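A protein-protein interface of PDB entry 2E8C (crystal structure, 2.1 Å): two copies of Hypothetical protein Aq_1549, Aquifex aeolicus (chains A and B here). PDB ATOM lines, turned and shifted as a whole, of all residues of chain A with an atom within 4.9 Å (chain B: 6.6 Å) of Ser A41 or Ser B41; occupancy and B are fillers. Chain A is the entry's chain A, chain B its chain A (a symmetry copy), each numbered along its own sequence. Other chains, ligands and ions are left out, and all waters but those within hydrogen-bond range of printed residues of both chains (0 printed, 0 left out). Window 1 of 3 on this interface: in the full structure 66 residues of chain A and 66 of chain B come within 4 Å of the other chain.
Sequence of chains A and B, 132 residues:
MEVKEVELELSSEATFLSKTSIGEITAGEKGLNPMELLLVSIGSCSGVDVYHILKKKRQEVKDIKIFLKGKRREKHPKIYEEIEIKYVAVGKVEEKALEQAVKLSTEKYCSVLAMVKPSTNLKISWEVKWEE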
ATOM      1  N   PRO A  34       8.798  24.179 -12.563  1.00  0.00           N
ATOM      2  CA  PRO A  34       7.545  23.918 -11.838  1.00  0.00           C
ATOM      3  C   PRO A  34       7.478  24.448 -10.404  1.00  0.00           C
ATOM      4  O   PRO A  34       6.499  25.073 -10.023  1.00  0.00           O
ATOM      5  CB  PRO A  34       7.428  22.398 -11.899  1.00  0.00           C
ATOM      6  CG  PRO A  34       8.028  22.090 -13.251  1.00  0.00           C
ATOM      7  CD  PRO A  34       9.269  22.959 -13.245  1.00  0.00           C
ATOM      8  N   LEU A  37       7.352  28.104 -10.336  1.00  0.00           N
ATOM      9  CA  LEU A  37       6.018  28.524 -10.761  1.00  0.00           C
ATOM     10  C   LEU A  37       5.028  28.472  -9.601  1.00  0.00           C
ATOM     11  O   LEU A  37       4.069  29.249  -9.557  1.00  0.00           O
ATOM     12  CB  LEU A  37       5.494  27.642 -11.901  1.00  0.00           C
ATOM     13  CG  LEU A  37       5.920  28.037 -13.311  1.00  0.00           C
ATOM     14  CD1 LEU A  37       5.214  27.132 -14.322  1.00  0.00           C
ATOM     15  CD2 LEU A  37       5.552  29.507 -13.551  1.00  0.00           C
ATOM     16  N   LEU A  38       5.241  27.536  -8.681  1.00  0.00           N
ATOM     17  CA  LEU A  38       4.365  27.429  -7.516  1.00  0.00           C
ATOM     18  C   LEU A  38       4.534  28.712  -6.701  1.00  0.00           C
ATOM     19  O   LEU A  38       3.557  29.299  -6.229  1.00  0.00           O
ATOM     20  CB  LEU A  38       4.732  26.205  -6.659  1.00  0.00           C
ATOM     21  CG  LEU A  38       4.014  26.118  -5.296  1.00  0.00           C
ATOM     22  CD1 LEU A  38       2.517  26.098  -5.505  1.00  0.00           C
ATOM     23  CD2 LEU A  38       4.461  24.873  -4.538  1.00  0.00           C
ATOM     24  N   LEU A  39       5.779  29.155  -6.552  1.00  0.00           N
ATOM     25  CA  LEU A  39       6.059  30.383  -5.808  1.00  0.00           C
ATOM     26  C   LEU A  39       5.450  31.594  -6.512  1.00  0.00           C
ATOM     27  O   LEU A  39       4.953  32.517  -5.860  1.00  0.00           O
ATOM     28  CB  LEU A  39       7.569  30.576  -5.643  1.00  0.00           C
ATOM     29  CG  LEU A  39       8.271  29.569  -4.726  1.00  0.00           C
ATOM     30  CD1 LEU A  39       9.749  29.892  -4.654  1.00  0.00           C
ATOM     31  CD2 LEU A  39       7.656  29.624  -3.329  1.00  0.00           C
ATOM     32  N   VAL A  40       5.490  31.593  -7.845  1.00  0.00           N
ATOM     33  CA  VAL A  40       4.916  32.695  -8.607  1.00  0.00           C
ATOM     34  C   VAL A  40       3.407  32.688  -8.393  1.00  0.00           C
ATOM     35  O   VAL A  40       2.778  33.741  -8.280  1.00  0.00           O
ATOM     36  CB  VAL A  40       5.189  32.559 -10.127  1.00  0.00           C
ATOM     37  CG1 VAL A  40       4.384  33.621 -10.898  1.00  0.00           C
ATOM     38  CG2 VAL A  40       6.680  32.720 -10.405  1.00  0.00           C
ATOM     39  N   SER A  41       2.838  31.487  -8.350  1.00  0.00           N
ATOM     40  CA  SER A  41       1.405  31.310  -8.142  1.00  0.00           C
ATOM     41  C   SER A  41       0.999  31.871  -6.789  1.00  0.00           C
ATOM     42  O   SER A  41      -0.014  32.552  -6.669  1.00  0.00           O
ATOM     43  CB  SER A  41       1.044  29.824  -8.192  1.00  0.00           C
ATOM     44  OG  SER A  41       1.478  29.254  -9.416  1.00  0.00           O
ATOM     45  N   ILE A  42       1.795  31.561  -5.771  1.00  0.00           N
ATOM     46  CA  ILE A  42       1.540  32.030  -4.417  1.00  0.00           C
ATOM     47  C   ILE A  42       1.698  33.550  -4.342  1.00  0.00           C
ATOM     48  O   ILE A  42       0.820  34.255  -3.847  1.00  0.00           O
ATOM     49  CB  ILE A  42       2.525  31.374  -3.417  1.00  0.00           C
ATOM     50  CG1 ILE A  42       2.273  29.860  -3.354  1.00  0.00           C
ATOM     51  CG2 ILE A  42       2.384  32.021  -2.047  1.00  0.00           C
ATOM     52  CD1 ILE A  42       3.330  29.076  -2.566  1.00  0.00           C
ATOM     53  N   GLY A  43       2.816  34.048  -4.855  1.00  0.00           N
ATOM     54  CA  GLY A  43       3.064  35.476  -4.823  1.00  0.00           C
ATOM     55  C   GLY A  43       2.031  36.330  -5.539  1.00  0.00           C
ATOM     56  O   GLY A  43       1.609  37.364  -5.013  1.00  0.00           O
ATOM     57  N   SER A  44       1.620  35.907  -6.733  1.00  0.00           N
ATOM     58  CA  SER A  44       0.644  36.665  -7.522  1.00  0.00           C
ATOM     59  C   SER A  44      -0.742  36.637  -6.888  1.00  0.00           C
ATOM     60  O   SER A  44      -1.450  37.648  -6.862  1.00  0.00           O
ATOM     61  CB  SER A  44       0.583  36.121  -8.956  1.00  0.00           C
ATOM     62  OG  SER A  44       0.367  34.718  -8.981  1.00  0.00           O
ATOM     63  N   CYS A  45      -1.126  35.471  -6.381  1.00  0.00           N
ATOM     64  CA  CYS A  45      -2.411  35.302  -5.709  1.00  0.00           C
ATOM     65  C   CYS A  45      -2.485  36.283  -4.552  1.00  0.00           C
ATOM     66  O   CYS A  45      -3.415  37.076  -4.451  1.00  0.00           O
ATOM     67  CB  CYS A  45      -2.500  33.887  -5.173  1.00  0.00           C
ATOM     68  SG  CYS A  45      -3.856  33.364  -4.062  1.00  0.00           S
ATOM     69  N   VAL A 112      -4.297  30.021  -3.336  1.00  0.00           N
ATOM     70  CA  VAL A 112      -3.105  29.210  -3.581  1.00  0.00           C
ATOM     71  C   VAL A 112      -2.354  28.946  -2.285  1.00  0.00           C
ATOM     72  O   VAL A 112      -2.015  27.803  -1.973  1.00  0.00           O
ATOM     73  CB  VAL A 112      -2.138  29.909  -4.565  1.00  0.00           C
ATOM     74  CG1 VAL A 112      -0.910  29.028  -4.811  1.00  0.00           C
ATOM     75  CG2 VAL A 112      -2.860  30.210  -5.879  1.00  0.00           C
ATOM     76  N   LEU B   8       8.523  39.228  -7.599  1.00  0.00           N
ATOM     77  CA  LEU B   8       7.413  39.835  -8.315  1.00  0.00           C
ATOM     78  C   LEU B   8       7.392  41.346  -8.134  1.00  0.00           C
ATOM     79  O   LEU B   8       7.788  41.874  -7.091  1.00  0.00           O
ATOM     80  CB  LEU B   8       6.080  39.253  -7.830  1.00  0.00           C
ATOM     81  CG  LEU B   8       5.674  37.853  -8.307  1.00  0.00           C
ATOM     82  CD1 LEU B   8       6.702  36.828  -7.874  1.00  0.00           C
ATOM     83  CD2 LEU B   8       4.302  37.510  -7.744  1.00  0.00           C
ATOM     84  N   ALA B  27       1.662  37.633 -14.034  1.00  0.00           N
ATOM     85  CA  ALA B  27       0.703  36.846 -13.271  1.00  0.00           C
ATOM     86  C   ALA B  27      -0.179  37.779 -12.460  1.00  0.00           C
ATOM     87  O   ALA B  27       0.314  38.677 -11.771  1.00  0.00           O
ATOM     88  CB  ALA B  27       1.440  35.883 -12.345  1.00  0.00           C
ATOM     89  N   ASN B  33      -3.690  33.802 -14.747  1.00  0.00           N
ATOM     90  CA  ASN B  33      -4.479  33.685 -13.530  1.00  0.00           C
ATOM     91  C   ASN B  33      -3.710  32.830 -12.515  1.00  0.00           C
ATOM     92  O   ASN B  33      -3.256  31.736 -12.835  1.00  0.00           O
ATOM     93  CB  ASN B  33      -5.844  33.061 -13.850  1.00  0.00           C
ATOM     94  CG  ASN B  33      -6.643  32.733 -12.602  1.00  0.00           C
ATOM     95  OD1 ASN B  33      -6.616  31.605 -12.116  1.00  0.00           O
ATOM     96  ND2 ASN B  33      -7.348  33.729 -12.069  1.00  0.00           N
ATOM     97  N   PRO B  34      -3.545  33.330 -11.280  1.00  0.00           N
ATOM     98  CA  PRO B  34      -2.826  32.621 -10.211  1.00  0.00           C
ATOM     99  C   PRO B  34      -3.262  31.175  -9.957  1.00  0.00           C
ATOM    100  O   PRO B  34      -2.427  30.288  -9.854  1.00  0.00           O
ATOM    101  CB  PRO B  34      -3.052  33.516  -8.997  1.00  0.00           C
ATOM    102  CG  PRO B  34      -3.065  34.893  -9.619  1.00  0.00           C
ATOM    103  CD  PRO B  34      -3.947  34.677 -10.832  1.00  0.00           C
ATOM    104  N   MET B  35      -4.563  30.936  -9.844  1.00  0.00           N
ATOM    105  CA  MET B  35      -5.041  29.578  -9.592  1.00  0.00           C
ATOM    106  C   MET B  35      -4.881  28.663 -10.812  1.00  0.00           C
ATOM    107  O   MET B  35      -4.775  27.449 -10.661  1.00  0.00           O
ATOM    108  CB  MET B  35      -6.492  29.607  -9.101  1.00  0.00           C
ATOM    109  CG  MET B  35      -6.608  29.929  -7.589  1.00  0.00           C
ATOM    110  SD  MET B  35      -6.038  28.560  -6.492  1.00  0.00           S
ATOM    111  CE  MET B  35      -7.612  27.715  -6.210  1.00  0.00           C
ATOM    112  N   GLU B  36      -4.873  29.226 -12.020  1.00  0.00           N
ATOM    113  CA  GLU B  36      -4.647  28.387 -13.196  1.00  0.00           C
ATOM    114  C   GLU B  36      -3.157  28.050 -13.205  1.00  0.00           C
ATOM    115  O   GLU B  36      -2.762  26.963 -13.623  1.00  0.00           O
ATOM    116  CB  GLU B  36      -5.023  29.109 -14.496  1.00  0.00           C
ATOM    117  CG  GLU B  36      -6.515  29.376 -14.660  1.00  0.00           C
ATOM    118  CD  GLU B  36      -6.873  29.903 -16.041  1.00  0.00           C
ATOM    119  OE1 GLU B  36      -5.958  30.309 -16.785  1.00  0.00           O
ATOM    120  OE2 GLU B  36      -8.075  29.916 -16.382  1.00  0.00           O
ATOM    121  N   LEU B  37      -2.329  28.989 -12.738  1.00  0.00           N
ATOM    122  CA  LEU B  37      -0.884  28.769 -12.682  1.00  0.00           C
ATOM    123  C   LEU B  37      -0.533  27.659 -11.696  1.00  0.00           C
ATOM    124  O   LEU B  37       0.465  26.954 -11.873  1.00  0.00           O
ATOM    125  CB  LEU B  37      -0.143  30.048 -12.275  1.00  0.00           C
ATOM    126  CG  LEU B  37       0.186  31.025 -13.399  1.00  0.00           C
ATOM    127  CD1 LEU B  37       1.026  32.174 -12.838  1.00  0.00           C
ATOM    128  CD2 LEU B  37       0.953  30.282 -14.501  1.00  0.00           C
ATOM    129  N   LEU B  38      -1.333  27.526 -10.643  1.00  0.00           N
ATOM    130  CA  LEU B  38      -1.096  26.470  -9.661  1.00  0.00           C
ATOM    131  C   LEU B  38      -1.296  25.132 -10.374  1.00  0.00           C
ATOM    132  O   LEU B  38      -0.510  24.196 -10.203  1.00  0.00           O
ATOM    133  CB  LEU B  38      -2.071  26.588  -8.476  1.00  0.00           C
ATOM    134  CG  LEU B  38      -2.053  25.402  -7.489  1.00  0.00           C
ATOM    135  CD1 LEU B  38      -0.662  25.229  -6.922  1.00  0.00           C
ATOM    136  CD2 LEU B  38      -3.059  25.629  -6.366  1.00  0.00           C
ATOM    137  N   LEU B  39      -2.342  25.051 -11.192  1.00  0.00           N
ATOM    138  CA  LEU B  39      -2.620  23.827 -11.942  1.00  0.00           C
ATOM    139  C   LEU B  39      -1.503  23.539 -12.944  1.00  0.00           C
ATOM    140  O   LEU B  39      -1.136  22.381 -13.161  1.00  0.00           O
ATOM    141  CB  LEU B  39      -3.962  23.939 -12.670  1.00  0.00           C
ATOM    142  CG  LEU B  39      -5.204  23.963 -11.772  1.00  0.00           C
ATOM    143  CD1 LEU B  39      -6.449  24.065 -12.630  1.00  0.00           C
ATOM    144  CD2 LEU B  39      -5.257  22.693 -10.926  1.00  0.00           C
ATOM    145  N   VAL B  40      -0.965  24.594 -13.557  1.00  0.00           N
ATOM    146  CA  VAL B  40       0.122  24.424 -14.514  1.00  0.00           C
ATOM    147  C   VAL B  40       1.343  23.907 -13.762  1.00  0.00           C
ATOM    148  O   VAL B  40       2.088  23.066 -14.266  1.00  0.00           O
ATOM    149  CB  VAL B  40       0.506  25.757 -15.205  1.00  0.00           C
ATOM    150  CG1 VAL B  40       1.788  25.562 -16.035  1.00  0.00           C
ATOM    151  CG2 VAL B  40      -0.637  26.230 -16.097  1.00  0.00           C
ATOM    152  N   SER B  41       1.541  24.432 -12.557  1.00  0.00           N
ATOM    153  CA  SER B  41       2.659  24.037 -11.708  1.00  0.00           C
ATOM    154  C   SER B  41       2.561  22.559 -11.368  1.00  0.00           C
ATOM    155  O   SER B  41       3.551  21.836 -11.411  1.00  0.00           O
ATOM    156  CB  SER B  41       2.649  24.847 -10.410  1.00  0.00           C
ATOM    157  OG  SER B  41       2.664  26.235 -10.698  1.00  0.00           O
ATOM    158  N   ILE B  42       1.356  22.124 -11.012  1.00  0.00           N
ATOM    159  CA  ILE B  42       1.105  20.734 -10.664  1.00  0.00           C
ATOM    160  C   ILE B  42       1.289  19.838 -11.890  1.00  0.00           C
ATOM    161  O   ILE B  42       2.006  18.838 -11.843  1.00  0.00           O
ATOM    162  CB  ILE B  42      -0.338  20.558 -10.127  1.00  0.00           C
ATOM    163  CG1 ILE B  42      -0.498  21.321  -8.804  1.00  0.00           C
ATOM    164  CG2 ILE B  42      -0.654  19.078  -9.961  1.00  0.00           C
ATOM    165  CD1 ILE B  42      -1.942  21.400  -8.292  1.00  0.00           C
ATOM    166  N   GLY B  43       0.652  20.214 -12.992  1.00  0.00           N
ATOM    167  CA  GLY B  43       0.755  19.424 -14.204  1.00  0.00           C
ATOM    168  C   GLY B  43       2.163  19.254 -14.748  1.00  0.00           C
ATOM    169  O   GLY B  43       2.546  18.148 -15.141  1.00  0.00           O
ATOM    170  N   SER B  44       2.937  20.337 -14.774  1.00  0.00           N
ATOM    171  CA  SER B  44       4.305  20.292 -15.300  1.00  0.00           C
ATOM    172  C   SER B  44       5.233  19.487 -14.398  1.00  0.00           C
ATOM    173  O   SER B  44       6.076  18.720 -14.873  1.00  0.00           O
ATOM    174  CB  SER B  44       4.849  21.715 -15.489  1.00  0.00           C
ATOM    175  OG  SER B  44       4.721  22.491 -14.307  1.00  0.00           O
ATOM    176  N   CYS B  45       5.077  19.671 -13.092  1.00  0.00           N
ATOM    177  CA  CYS B  45       5.870  18.942 -12.105  1.00  0.00           C
ATOM    178  C   CYS B  45       5.664  17.454 -12.325  1.00  0.00           C
ATOM    179  O   CYS B  45       6.616  16.701 -12.500  1.00  0.00           O
ATOM    180  CB  CYS B  45       5.386  19.316 -10.718  1.00  0.00           C
ATOM    181  SG  CYS B  45       5.967  18.430  -9.227  1.00  0.00           S
ATOM    182  N   SER B  46       4.406  17.037 -12.314  1.00  0.00           N
ATOM    183  CA  SER B  46       4.079  15.633 -12.503  1.00  0.00           C
ATOM    184  C   SER B  46       4.477  15.218 -13.915  1.00  0.00           C
ATOM    185  O   SER B  46       5.033  14.142 -14.118  1.00  0.00           O
ATOM    186  CB  SER B  46       2.583  15.408 -12.281  1.00  0.00           C
ATOM    187  OG  SER B  46       2.266  14.024 -12.328  1.00  0.00           O
ATOM    188  N   CYS B 110       6.448  14.057  -7.498  1.00  0.00           N
ATOM    189  CA  CYS B 110       6.101  15.455  -7.728  1.00  0.00           C
ATOM    190  C   CYS B 110       5.891  16.286  -6.456  1.00  0.00           C
ATOM    191  O   CYS B 110       4.936  16.095  -5.692  1.00  0.00           O
ATOM    192  CB  CYS B 110       4.904  15.595  -8.696  1.00  0.00           C
ATOM    193  SG  CYS B 110       4.334  17.320  -8.657  1.00  0.00           S
ATOM    194  N   VAL B 112       5.259  19.681  -6.092  1.00  0.00           N
ATOM    195  CA  VAL B 112       4.136  20.618  -6.079  1.00  0.00           C
ATOM    196  C   VAL B 112       2.862  19.930  -5.616  1.00  0.00           C
ATOM    197  O   VAL B 112       2.165  20.422  -4.727  1.00  0.00           O
ATOM    198  CB  VAL B 112       3.880  21.213  -7.484  1.00  0.00           C
ATOM    199  CG1 VAL B 112       2.710  22.199  -7.432  1.00  0.00           C
ATOM    200  CG2 VAL B 112       5.146  21.901  -7.996  1.00  0.00           C
ATOM    201  N   LEU B 113       2.566  18.784  -6.221  1.00  0.00           N
ATOM    202  CA  LEU B 113       1.367  18.027  -5.889  1.00  0.00           C
ATOM    203  C   LEU B 113       1.340  17.562  -4.434  1.00  0.00           C
ATOM    204  O   LEU B 113       0.287  17.550  -3.799  1.00  0.00           O
ATOM    205  CB  LEU B 113       1.241  16.817  -6.816  1.00  0.00           C
ATOM    206  CG  LEU B 113      -0.089  16.074  -6.722  1.00  0.00           C
ATOM    207  CD1 LEU B 113      -1.234  17.039  -6.956  1.00  0.00           C
ATOM    208  CD2 LEU B 113      -0.115  14.952  -7.748  1.00  0.00           C
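OG of Ser B41 lies within hydrogen-bond range of OG of Ser A41 (3.5 Å).
OD1 of Asn B33 sits at hydrogen-bond distance from N of Met B35 (3.1 Å). The side-chain sulfur of Cys B110 is disulfide-bonded to the side-chain sulfur of Cys B45 (2.1 Å). The backbone carbonyl oxygen (O) of Ser A41 lies within hydrogen-bond range of the side-chain hydroxyl (OG) of Ser A44. The side-chain hydroxyl (OG) of Ser B41 is in hydrogen-bond range of the backbone carbonyl oxygen (O) of Leu B37. The side-chain hydroxyl (OG) of Ser B44 lies within hydrogen-bond range of the backbone carbonyl oxygen (O) of Ser B41 (3.2 Å). OG of Ser B44 lies within hydrogen-bond range of O of Val B40, 2.7 Å away.
CG of Pro A34 touches OG of Ser B44, 3.5 Å away. Pro A34 touches Cys B45. Ser B41 touches Leu A38. Ala B27 touches Val A40. Ser A41 touches Pro B34 (CB to O, 3.9 Å). Leu B38 touches Ser A41. Ser A44 touches Ala B27. CG of Pro B34 touches OG of Ser A44, at 3.5 Å. CG2 of Val A112 touches O of Pro B34, at 3.999 Å. CG2 of Val A112 touches SD of Met B35 (3.6 Å).
Ser A41 touches just these residues of chain B: Pro B34 (3.9 Å), Leu B37 (3.4 Å), Leu B38 (3.5 Å) and Ser B41 (3.5 Å). Ser B41 touches four residues of chain A. Printed residues of chain B within 4 Å of Leu A37: Ser B41 (3.4 Å). Of the printed residues of chain A, Leu B37 touches Ser A41. Of the printed residues of chain A, Ser B44 touches Pro A34 (3.5 Å). Of the printed residues of chain A, Ala B27 touches Val A40 and Ser A44. Of the printed residues of chain A, Leu B38 touches Leu A38 and Ser A41. Glu B36 touches none of the printed residues of chain A. The nearest printed residue of chain B that does not touch Ser A44 is Leu B37 (4.7 Å).
Hydrophobic or aromatic side chains of chain A within 4 Å of the printed part of chain B: Pro A34, Leu A37, Leu A38, Val A40 and Val A112. Printed residues of chain B that touch a printed residue of chain A: Leu B8, Ala B27, Pro B34, Met B35, Leu B37, Leu B38, Ser B41, Ser B44 and Cys B45. Hydrophobic or aromatic side chains of chain B that line the printed part of chain A: Leu B8, Ala B27, Pro B34, Met B35, Leu B37 and Leu B38.
Pro A34 touches Ser B41, and with the chains exchanged Ser A41 touches Pro B34. Pro A34 touches Cys B45, and with the chains exchanged Cys A45 touches Pro B34. Leu B38 touches its own counterpart, Leu A38. Leu A38 touches Ser B41, and with the chains exchanged Ser A41 touches Leu B38. 11 positions are printed for both chains.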
